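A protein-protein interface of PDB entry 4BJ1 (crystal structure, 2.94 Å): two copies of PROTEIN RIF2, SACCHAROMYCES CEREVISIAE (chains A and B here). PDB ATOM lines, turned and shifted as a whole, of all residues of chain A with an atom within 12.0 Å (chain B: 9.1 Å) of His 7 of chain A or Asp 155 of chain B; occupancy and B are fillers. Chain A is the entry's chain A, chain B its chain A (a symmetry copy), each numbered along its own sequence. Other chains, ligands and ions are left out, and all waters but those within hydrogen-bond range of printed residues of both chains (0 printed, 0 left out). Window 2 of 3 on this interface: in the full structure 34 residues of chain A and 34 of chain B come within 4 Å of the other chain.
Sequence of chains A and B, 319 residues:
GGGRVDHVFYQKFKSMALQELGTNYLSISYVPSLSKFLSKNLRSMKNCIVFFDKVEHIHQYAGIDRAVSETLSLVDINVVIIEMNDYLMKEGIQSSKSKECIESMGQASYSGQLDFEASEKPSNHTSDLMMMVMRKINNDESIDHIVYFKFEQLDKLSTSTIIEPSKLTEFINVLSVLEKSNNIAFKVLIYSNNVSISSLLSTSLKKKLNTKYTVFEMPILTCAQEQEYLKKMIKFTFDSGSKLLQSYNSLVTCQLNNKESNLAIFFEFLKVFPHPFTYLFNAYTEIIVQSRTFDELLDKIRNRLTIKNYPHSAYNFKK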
ATOM      1  N   HIS A   7       6.658   7.998 -24.208  1.00  0.00           N
ATOM      2  CA  HIS A   7       6.526   9.341 -23.647  1.00  0.00           C
ATOM      3  C   HIS A   7       7.889  10.020 -23.307  1.00  0.00           C
ATOM      4  O   HIS A   7       7.994  11.249 -23.427  1.00  0.00           O
ATOM      5  CB  HIS A   7       5.580   9.343 -22.434  1.00  0.00           C
ATOM      6  N   VAL A   8       8.924   9.242 -22.889  1.00  0.00           N
ATOM      7  CA  VAL A   8      10.239   9.839 -22.571  1.00  0.00           C
ATOM      8  C   VAL A   8      11.290   9.346 -23.551  1.00  0.00           C
ATOM      9  O   VAL A   8      12.002   8.369 -23.284  1.00  0.00           O
ATOM     10  CB  VAL A   8      10.671   9.692 -21.095  1.00  0.00           C
ATOM     11  CG1 VAL A   8      11.909  10.556 -20.800  1.00  0.00           C
ATOM     12  CG2 VAL A   8       9.504  10.003 -20.133  1.00  0.00           C
ATOM     13  N   PHE A   9      11.379  10.044 -24.691  1.00  0.00           N
ATOM     14  CA  PHE A   9      12.232   9.702 -25.821  1.00  0.00           C
ATOM     15  C   PHE A   9      13.728   9.839 -25.504  1.00  0.00           C
ATOM     16  O   PHE A   9      14.381  10.880 -25.724  1.00  0.00           O
ATOM     17  CB  PHE A   9      11.786  10.474 -27.047  1.00  0.00           C
ATOM     18  CG  PHE A   9      10.318  10.235 -27.303  1.00  0.00           C
ATOM     19  CD1 PHE A   9       9.818   8.943 -27.450  1.00  0.00           C
ATOM     20  CD2 PHE A   9       9.425  11.296 -27.362  1.00  0.00           C
ATOM     21  CE1 PHE A   9       8.447   8.721 -27.668  1.00  0.00           C
ATOM     22  CE2 PHE A   9       8.059  11.073 -27.584  1.00  0.00           C
ATOM     23  CZ  PHE A   9       7.583   9.788 -27.746  1.00  0.00           C
ATOM     24  N   TYR A  10      14.241   8.750 -24.916  1.00  0.00           N
ATOM     25  CA  TYR A  10      15.621   8.614 -24.499  1.00  0.00           C
ATOM     26  C   TYR A  10      16.509   8.480 -25.737  1.00  0.00           C
ATOM     27  O   TYR A  10      17.596   9.041 -25.749  1.00  0.00           O
ATOM     28  CB  TYR A  10      15.788   7.443 -23.513  1.00  0.00           C
ATOM     29  CG  TYR A  10      17.212   7.244 -23.076  1.00  0.00           C
ATOM     30  CD1 TYR A  10      17.895   8.242 -22.383  1.00  0.00           C
ATOM     31  CD2 TYR A  10      17.919   6.105 -23.444  1.00  0.00           C
ATOM     32  CE1 TYR A  10      19.248   8.110 -22.070  1.00  0.00           C
ATOM     33  CE2 TYR A  10      19.280   5.965 -23.145  1.00  0.00           C
ATOM     34  CZ  TYR A  10      19.938   6.971 -22.462  1.00  0.00           C
ATOM     35  OH  TYR A  10      21.259   6.806 -22.135  1.00  0.00           O
ATOM     36  N   GLN A  11      16.016   7.834 -26.805  1.00  0.00           N
ATOM     37  CA  GLN A  11      16.737   7.711 -28.064  1.00  0.00           C
ATOM     38  C   GLN A  11      17.168   9.087 -28.607  1.00  0.00           C
ATOM     39  O   GLN A  11      18.257   9.204 -29.160  1.00  0.00           O
ATOM     40  CB  GLN A  11      15.879   6.969 -29.091  1.00  0.00           C
ATOM     41  CG  GLN A  11      16.623   6.568 -30.350  1.00  0.00           C
ATOM     42  CD  GLN A  11      17.763   5.654 -30.024  1.00  0.00           C
ATOM     43  OE1 GLN A  11      17.584   4.610 -29.382  1.00  0.00           O
ATOM     44  NE2 GLN A  11      18.964   6.053 -30.434  1.00  0.00           N
ATOM     45  N   LYS A  12      16.336  10.122 -28.421  1.00  0.00           N
ATOM     46  CA  LYS A  12      16.664  11.484 -28.841  1.00  0.00           C
ATOM     47  C   LYS A  12      17.861  11.997 -28.019  1.00  0.00           C
ATOM     48  O   LYS A  12      18.824  12.484 -28.615  1.00  0.00           O
ATOM     49  CB  LYS A  12      15.449  12.428 -28.738  1.00  0.00           C
ATOM     50  CG  LYS A  12      15.781  13.833 -29.221  1.00  0.00           C
ATOM     51  CD  LYS A  12      14.544  14.672 -29.561  1.00  0.00           C
ATOM     52  CE  LYS A  12      14.022  15.540 -28.438  1.00  0.00           C
ATOM     53  NZ  LYS A  12      15.044  16.490 -27.947  1.00  0.00           N
ATOM     54  N   PHE A  13      17.820  11.824 -26.663  1.00  0.00           N
ATOM     55  CA  PHE A  13      18.876  12.209 -25.735  1.00  0.00           C
ATOM     56  C   PHE A  13      20.126  11.416 -26.050  1.00  0.00           C
ATOM     57  O   PHE A  13      21.173  12.015 -26.280  1.00  0.00           O
ATOM     58  CB  PHE A  13      18.451  11.962 -24.278  1.00  0.00           C
ATOM     59  CG  PHE A  13      19.460  12.488 -23.295  1.00  0.00           C
ATOM     60  CD1 PHE A  13      19.469  13.830 -22.933  1.00  0.00           C
ATOM     61  CD2 PHE A  13      20.476  11.666 -22.806  1.00  0.00           C
ATOM     62  CE1 PHE A  13      20.467  14.338 -22.084  1.00  0.00           C
ATOM     63  CE2 PHE A  13      21.472  12.174 -21.954  1.00  0.00           C
ATOM     64  CZ  PHE A  13      21.452  13.501 -21.588  1.00  0.00           C
ATOM     65  N   ASP A 239      19.415  21.119 -26.792  1.00  0.00           N
ATOM     66  CA  ASP A 239      18.111  21.398 -26.131  1.00  0.00           C
ATOM     67  C   ASP A 239      18.345  22.254 -24.890  1.00  0.00           C
ATOM     68  O   ASP A 239      18.073  21.816 -23.762  1.00  0.00           O
ATOM     69  CB  ASP A 239      17.290  20.133 -25.762  1.00  0.00           C
ATOM     70  CG  ASP A 239      17.172  19.078 -26.836  1.00  0.00           C
ATOM     71  OD1 ASP A 239      16.914  19.448 -27.998  1.00  0.00           O
ATOM     72  OD2 ASP A 239      17.325  17.865 -26.507  1.00  0.00           O
ATOM     73  N   SER A 242      15.825  22.866 -21.628  1.00  0.00           N
ATOM     74  CA  SER A 242      14.981  21.693 -21.388  1.00  0.00           C
ATOM     75  C   SER A 242      15.234  21.070 -20.014  1.00  0.00           C
ATOM     76  O   SER A 242      16.379  21.057 -19.559  1.00  0.00           O
ATOM     77  CB  SER A 242      15.118  20.667 -22.509  1.00  0.00           C
ATOM     78  OG  SER A 242      16.319  19.920 -22.426  1.00  0.00           O
ATOM     79  N   LYS A 243      14.161  20.587 -19.347  1.00  0.00           N
ATOM     80  CA  LYS A 243      14.227  19.942 -18.025  1.00  0.00           C
ATOM     81  C   LYS A 243      15.023  18.628 -18.075  1.00  0.00           C
ATOM     82  O   LYS A 243      15.642  18.261 -17.081  1.00  0.00           O
ATOM     83  CB  LYS A 243      12.823  19.697 -17.449  1.00  0.00           C
ATOM     84  N   LEU A 244      15.031  17.944 -19.232  1.00  0.00           N
ATOM     85  CA  LEU A 244      15.771  16.706 -19.380  1.00  0.00           C
ATOM     86  C   LEU A 244      17.271  16.990 -19.378  1.00  0.00           C
ATOM     87  O   LEU A 244      18.038  16.207 -18.811  1.00  0.00           O
ATOM     88  CB  LEU A 244      15.333  15.985 -20.659  1.00  0.00           C
ATOM     89  CG  LEU A 244      15.770  14.530 -20.844  1.00  0.00           C
ATOM     90  CD1 LEU A 244      14.962  13.597 -19.986  1.00  0.00           C
ATOM     91  CD2 LEU A 244      15.543  14.105 -22.250  1.00  0.00           C
ATOM     92  N   ARG A 292      19.045   1.947 -21.591  1.00  0.00           N
ATOM     93  CA  ARG A 292      17.879   1.895 -22.463  1.00  0.00           C
ATOM     94  C   ARG A 292      16.812   2.929 -22.085  1.00  0.00           C
ATOM     95  O   ARG A 292      15.894   3.187 -22.867  1.00  0.00           O
ATOM     96  CB  ARG A 292      17.329   0.472 -22.529  1.00  0.00           C
ATOM     97  CG  ARG A 292      18.242  -0.450 -23.340  1.00  0.00           C
ATOM     98  CD  ARG A 292      17.576  -1.766 -23.694  1.00  0.00           C
ATOM     99  NE  ARG A 292      16.427  -1.583 -24.584  1.00  0.00           N
ATOM    100  CZ  ARG A 292      15.515  -2.516 -24.830  1.00  0.00           C
ATOM    101  NH1 ARG A 292      15.609  -3.713 -24.260  1.00  0.00           N
ATOM    102  NH2 ARG A 292      14.497  -2.261 -25.643  1.00  0.00           N
ATOM    103  N   THR A 293      16.943   3.527 -20.887  1.00  0.00           N
ATOM    104  CA  THR A 293      16.054   4.581 -20.398  1.00  0.00           C
ATOM    105  C   THR A 293      16.864   5.702 -19.751  1.00  0.00           C
ATOM    106  O   THR A 293      18.029   5.490 -19.393  1.00  0.00           O
ATOM    107  CB  THR A 293      15.006   4.042 -19.446  1.00  0.00           C
ATOM    108  OG1 THR A 293      15.659   3.595 -18.264  1.00  0.00           O
ATOM    109  CG2 THR A 293      14.135   2.936 -20.059  1.00  0.00           C
ATOM    110  N   PHE A 294      16.247   6.898 -19.598  1.00  0.00           N
ATOM    111  CA  PHE A 294      16.911   8.042 -18.976  1.00  0.00           C
ATOM    112  C   PHE A 294      17.274   7.755 -17.505  1.00  0.00           C
ATOM    113  O   PHE A 294      18.362   8.138 -17.040  1.00  0.00           O
ATOM    114  CB  PHE A 294      16.069   9.318 -19.107  1.00  0.00           C
ATOM    115  CG  PHE A 294      16.807  10.571 -18.689  1.00  0.00           C
ATOM    116  CD1 PHE A 294      17.922  11.018 -19.405  1.00  0.00           C
ATOM    117  CD2 PHE A 294      16.406  11.293 -17.572  1.00  0.00           C
ATOM    118  CE1 PHE A 294      18.617  12.165 -19.003  1.00  0.00           C
ATOM    119  CE2 PHE A 294      17.084  12.453 -17.185  1.00  0.00           C
ATOM    120  CZ  PHE A 294      18.188  12.878 -17.896  1.00  0.00           C
ATOM    121  N   ASP A 295      16.383   7.021 -16.808  1.00  0.00           N
ATOM    122  CA  ASP A 295      16.562   6.648 -15.407  1.00  0.00           C
ATOM    123  C   ASP A 295      17.709   5.648 -15.230  1.00  0.00           C
ATOM    124  O   ASP A 295      18.507   5.783 -14.296  1.00  0.00           O
ATOM    125  CB  ASP A 295      15.243   6.179 -14.808  1.00  0.00           C
ATOM    126  CG  ASP A 295      14.150   7.209 -15.033  1.00  0.00           C
ATOM    127  OD1 ASP A 295      13.578   7.237 -16.160  1.00  0.00           O
ATOM    128  OD2 ASP A 295      13.938   8.055 -14.134  1.00  0.00           O
ATOM    129  N   VAL B  55       5.251  13.024 -38.320  1.00  0.00           N
ATOM    130  CA  VAL B  55       6.517  12.796 -37.582  1.00  0.00           C
ATOM    131  C   VAL B  55       6.278  11.436 -36.919  1.00  0.00           C
ATOM    132  O   VAL B  55       5.730  11.343 -35.809  1.00  0.00           O
ATOM    133  CB  VAL B  55       6.956  13.931 -36.595  1.00  0.00           C
ATOM    134  CG1 VAL B  55       8.193  13.507 -35.796  1.00  0.00           C
ATOM    135  CG2 VAL B  55       7.237  15.237 -37.338  1.00  0.00           C
ATOM    136  N   GLU B  56       6.557  10.378 -37.708  1.00  0.00           N
ATOM    137  CA  GLU B  56       6.239   8.991 -37.389  1.00  0.00           C
ATOM    138  C   GLU B  56       7.340   8.227 -36.747  1.00  0.00           C
ATOM    139  O   GLU B  56       7.157   7.061 -36.368  1.00  0.00           O
ATOM    140  CB  GLU B  56       5.772   8.271 -38.650  1.00  0.00           C
ATOM    141  CG  GLU B  56       4.392   8.718 -39.107  1.00  0.00           C
ATOM    142  CD  GLU B  56       4.177   8.638 -40.603  1.00  0.00           C
ATOM    143  OE1 GLU B  56       5.066   8.116 -41.318  1.00  0.00           O
ATOM    144  OE2 GLU B  56       3.111   9.105 -41.061  1.00  0.00           O
ATOM    145  N   ILE B  58      11.039   8.410 -34.174  1.00  0.00           N
ATOM    146  CA  ILE B  58      11.854   9.110 -33.201  1.00  0.00           C
ATOM    147  C   ILE B  58      13.096   9.717 -33.879  1.00  0.00           C
ATOM    148  O   ILE B  58      13.482  10.832 -33.530  1.00  0.00           O
ATOM    149  CB  ILE B  58      12.154   8.247 -31.951  1.00  0.00           C
ATOM    150  CG1 ILE B  58      12.555   9.133 -30.785  1.00  0.00           C
ATOM    151  CG2 ILE B  58      13.140   7.112 -32.213  1.00  0.00           C
ATOM    152  CD1 ILE B  58      11.487  10.082 -30.522  1.00  0.00           C
ATOM    153  N   TYR B  61      11.986  13.131 -35.366  1.00  0.00           N
ATOM    154  CA  TYR B  61      11.804  14.069 -34.268  1.00  0.00           C
ATOM    155  C   TYR B  61      13.158  14.609 -33.799  1.00  0.00           C
ATOM    156  O   TYR B  61      13.326  15.838 -33.738  1.00  0.00           O
ATOM    157  CB  TYR B  61      11.070  13.370 -33.118  1.00  0.00           C
ATOM    158  CG  TYR B  61      10.896  14.207 -31.871  1.00  0.00           C
ATOM    159  CD1 TYR B  61      10.528  15.555 -31.951  1.00  0.00           C
ATOM    160  CD2 TYR B  61      11.031  13.641 -30.604  1.00  0.00           C
ATOM    161  CE1 TYR B  61      10.394  16.338 -30.808  1.00  0.00           C
ATOM    162  CE2 TYR B  61      10.837  14.398 -29.453  1.00  0.00           C
ATOM    163  CZ  TYR B  61      10.533  15.749 -29.560  1.00  0.00           C
ATOM    164  OH  TYR B  61      10.396  16.506 -28.428  1.00  0.00           O
ATOM    165  N   ASN B  85       4.277  20.627 -22.903  1.00  0.00           N
ATOM    166  CA  ASN B  85       3.834  19.245 -22.706  1.00  0.00           C
ATOM    167  C   ASN B  85       3.309  18.974 -21.318  1.00  0.00           C
ATOM    168  O   ASN B  85       2.160  18.539 -21.173  1.00  0.00           O
ATOM    169  CB  ASN B  85       4.941  18.290 -23.054  1.00  0.00           C
ATOM    170  CG  ASN B  85       5.094  18.202 -24.526  1.00  0.00           C
ATOM    171  OD1 ASN B  85       4.297  17.535 -25.187  1.00  0.00           O
ATOM    172  ND2 ASN B  85       6.056  18.954 -25.073  1.00  0.00           N
ATOM    173  N   GLU B 152       4.691  18.471 -27.892  1.00  0.00           N
ATOM    174  CA  GLU B 152       4.909  17.201 -28.567  1.00  0.00           C
ATOM    175  C   GLU B 152       3.757  16.203 -28.283  1.00  0.00           C
ATOM    176  O   GLU B 152       3.544  15.788 -27.138  1.00  0.00           O
ATOM    177  CB  GLU B 152       6.309  16.665 -28.192  1.00  0.00           C
ATOM    178  CG  GLU B 152       6.586  15.202 -28.522  1.00  0.00           C
ATOM    179  CD  GLU B 152       6.255  14.235 -27.397  1.00  0.00           C
ATOM    180  OE1 GLU B 152       6.852  14.375 -26.301  1.00  0.00           O
ATOM    181  OE2 GLU B 152       5.366  13.374 -27.591  1.00  0.00           O
ATOM    182  N   GLN B 153       3.020  15.831 -29.343  1.00  0.00           N
ATOM    183  CA  GLN B 153       1.887  14.910 -29.284  1.00  0.00           C
ATOM    184  C   GLN B 153       2.168  13.744 -30.260  1.00  0.00           C
ATOM    185  O   GLN B 153       1.451  13.580 -31.259  1.00  0.00           O
ATOM    186  CB  GLN B 153       0.589  15.684 -29.651  1.00  0.00           C
ATOM    187  N   LEU B 154       3.215  12.938 -29.969  1.00  0.00           N
ATOM    188  CA  LEU B 154       3.690  11.896 -30.886  1.00  0.00           C
ATOM    189  C   LEU B 154       3.217  10.449 -30.601  1.00  0.00           C
ATOM    190  O   LEU B 154       3.562   9.534 -31.360  1.00  0.00           O
ATOM    191  CB  LEU B 154       5.223  11.951 -30.991  1.00  0.00           C
ATOM    192  CG  LEU B 154       5.832  13.136 -31.739  1.00  0.00           C
ATOM    193  CD1 LEU B 154       7.315  13.033 -31.758  1.00  0.00           C
ATOM    194  CD2 LEU B 154       5.362  13.200 -33.161  1.00  0.00           C
ATOM    195  N   ASP B 155       2.394  10.255 -29.558  1.00  0.00           N
ATOM    196  CA  ASP B 155       1.786   8.955 -29.231  1.00  0.00           C
ATOM    197  C   ASP B 155       0.244   9.075 -29.166  1.00  0.00           C
ATOM    198  O   ASP B 155      -0.423   8.174 -28.631  1.00  0.00           O
ATOM    199  CB  ASP B 155       2.374   8.346 -27.944  1.00  0.00           C
ATOM    200  CG  ASP B 155       3.705   7.630 -28.117  1.00  0.00           C
ATOM    201  OD1 ASP B 155       3.711   6.493 -28.662  1.00  0.00           O
ATOM    202  OD2 ASP B 155       4.723   8.157 -27.631  1.00  0.00           O
ATOM    203  N   LYS B 156      -0.312  10.183 -29.770  1.00  0.00           N
ATOM    204  CA  LYS B 156      -1.743  10.539 -29.895  1.00  0.00           C
ATOM    205  C   LYS B 156      -2.613   9.355 -30.350  1.00  0.00           C
ATOM    206  O   LYS B 156      -3.796   9.287 -30.021  1.00  0.00           O
ATOM    207  CB  LYS B 156      -1.921  11.718 -30.878  1.00  0.00           C
ATOM    208  CG  LYS B 156      -3.147  12.588 -30.577  1.00  0.00           C
ATOM    209  CD  LYS B 156      -3.634  13.437 -31.759  1.00  0.00           C
ATOM    210  CE  LYS B 156      -4.948  14.103 -31.404  1.00  0.00           C
ATOM    211  NZ  LYS B 156      -5.723  14.550 -32.597  1.00  0.00           N
ATOM    212  N   TYR B 191       4.566  19.105 -32.649  1.00  0.00           N
ATOM    213  CA  TYR B 191       4.995  17.867 -33.299  1.00  0.00           C
ATOM    214  C   TYR B 191       3.870  16.860 -33.114  1.00  0.00           C
ATOM    215  O   TYR B 191       3.533  16.530 -31.969  1.00  0.00           O
ATOM    216  CB  TYR B 191       6.277  17.314 -32.638  1.00  0.00           C
ATOM    217  CG  TYR B 191       7.481  18.237 -32.657  1.00  0.00           C
ATOM    218  CD1 TYR B 191       7.701  19.148 -31.630  1.00  0.00           C
ATOM    219  CD2 TYR B 191       8.453  18.129 -33.649  1.00  0.00           C
ATOM    220  CE1 TYR B 191       8.816  19.983 -31.629  1.00  0.00           C
ATOM    221  CE2 TYR B 191       9.587  18.938 -33.644  1.00  0.00           C
ATOM    222  CZ  TYR B 191       9.763  19.876 -32.639  1.00  0.00           C
ATOM    223  OH  TYR B 191      10.880  20.697 -32.635  1.00  0.00           O
ATOM    224  N   SER B 192       3.271  16.385 -34.230  1.00  0.00           N
ATOM    225  CA  SER B 192       2.177  15.409 -34.168  1.00  0.00           C
ATOM    226  C   SER B 192       2.291  14.249 -35.217  1.00  0.00           C
ATOM    227  O   SER B 192       3.246  14.240 -36.012  1.00  0.00           O
ATOM    228  CB  SER B 192       0.834  16.125 -34.253  1.00  0.00           C
ATOM    229  OG  SER B 192      -0.163  15.374 -33.573  1.00  0.00           O
ATOM    230  N   ASN B 193       1.330  13.260 -35.179  1.00  0.00           N
ATOM    231  CA  ASN B 193       1.208  12.064 -36.049  1.00  0.00           C
ATOM    232  C   ASN B 193       2.432  11.165 -36.006  1.00  0.00           C
ATOM    233  O   ASN B 193       2.514  10.301 -35.142  1.00  0.00           O
ATOM    234  CB  ASN B 193       0.839  12.405 -37.519  1.00  0.00           C
ATOM    235  CG  ASN B 193      -0.401  13.271 -37.741  1.00  0.00           C
ATOM    236  OD1 ASN B 193      -0.288  14.434 -38.150  1.00  0.00           O
ATOM    237  ND2 ASN B 193      -1.612  12.706 -37.574  1.00  0.00           N
ATOM    238  N   HIS B 275      11.110   0.988 -37.232  1.00  0.00           N
ATOM    239  CA  HIS B 275      11.992   2.118 -36.940  1.00  0.00           C
ATOM    240  C   HIS B 275      13.425   1.749 -37.351  1.00  0.00           C
ATOM    241  O   HIS B 275      14.249   1.465 -36.473  1.00  0.00           O
ATOM    242  CB  HIS B 275      11.873   2.503 -35.451  1.00  0.00           C
ATOM    243  CG  HIS B 275      10.493   2.945 -35.043  1.00  0.00           C
ATOM    244  ND1 HIS B 275      10.086   4.266 -35.170  1.00  0.00           N
ATOM    245  CD2 HIS B 275       9.484   2.231 -34.493  1.00  0.00           C
ATOM    246  CE1 HIS B 275       8.846   4.302 -34.718  1.00  0.00           C
ATOM    247  NE2 HIS B 275       8.445   3.106 -34.285  1.00  0.00           N
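Of the 15 printed residues of chain A, 4 touch a printed residue of chain B. Hydrophobic or aromatic side chains of chain A within 4 Å of the printed part of chain B: Phe 9. Of the 14 printed residues of chain B, 4 touch a printed residue of chain A. Hydrophobic or aromatic side chains of chain B within 4 Å of the printed part of chain A: Ile 58 and Tyr 61. Along chain B the printed residues that touch a printed residue of chain A span positions 58 to 155. Among the printed residues, no Asp or Glu carboxylate lies within 4 Å of a Lys or Arg side-chain nitrogen of the other chain.
No position is printed for both chains.
His 7 of chain A touches just one residue of chain B: Asp 155 (3.9 Å). Asp 155 of chain B touches just these residues of chain A: His 7 and Phe 9. No residue of chain B comes within 4 Å of Val 8 of chain A. No residue of chain A comes within 4 Å of Gln 153 of chain B. No residue of chain A comes within 4 Å of Leu 154 of chain B. No residue of chain A comes within 4 Å of Ser 192 of chain B. Printed residues of chain B within 4 Å of Gln 11 of chain A: Ile 58 (3.99 Å). Of the printed residues of chain B, Lys 12 of chain A touches Tyr 61. Of the printed residues of chain B, Phe 9 of chain A touches Ile 58 (3.4 Å), Tyr 61 (3.999 Å), Glu 152 (3.5 Å) and Asp 155 (3.3 Å). Of the printed residues of chain A, Tyr 61 of chain B touches Phe 9 and Lys 12. Val 55 of chain B touches none of the printed residues of chain A. The nearest residue of chain A that does not touch Asp 155 of chain B is Val 8 of chain A (6.4 Å).
Among the printed residues, pairs that only touch across the chains: His 7 of chain A with Asp 155 of chain B, Phe 9 of chain A with Ile 58 of chain B, Phe 9 of chain A with Tyr 61 of chain B, Phe 9 of chain A with Glu 152 of chain B, Phe 9 of chain A with Asp 155 of chain B, Gln 11 of chain A with Ile 58 of chain B and Lys 12 of chain A with Tyr 61 of chain B.
The side-chain carboxylate (OE2) of Glu 152 of chain B lies within hydrogen-bond range of the backbone NH (N) of Leu 154 of chain B. O of Glu 152 of chain B lies close to OD1 of Asn 85 of chain B (2.7 Å). The side-chain carboxylate of Asp 239 of chain A lies within salt-bridge range of the side-chain amino group of Lys 12 of chain A (3.0 Å).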
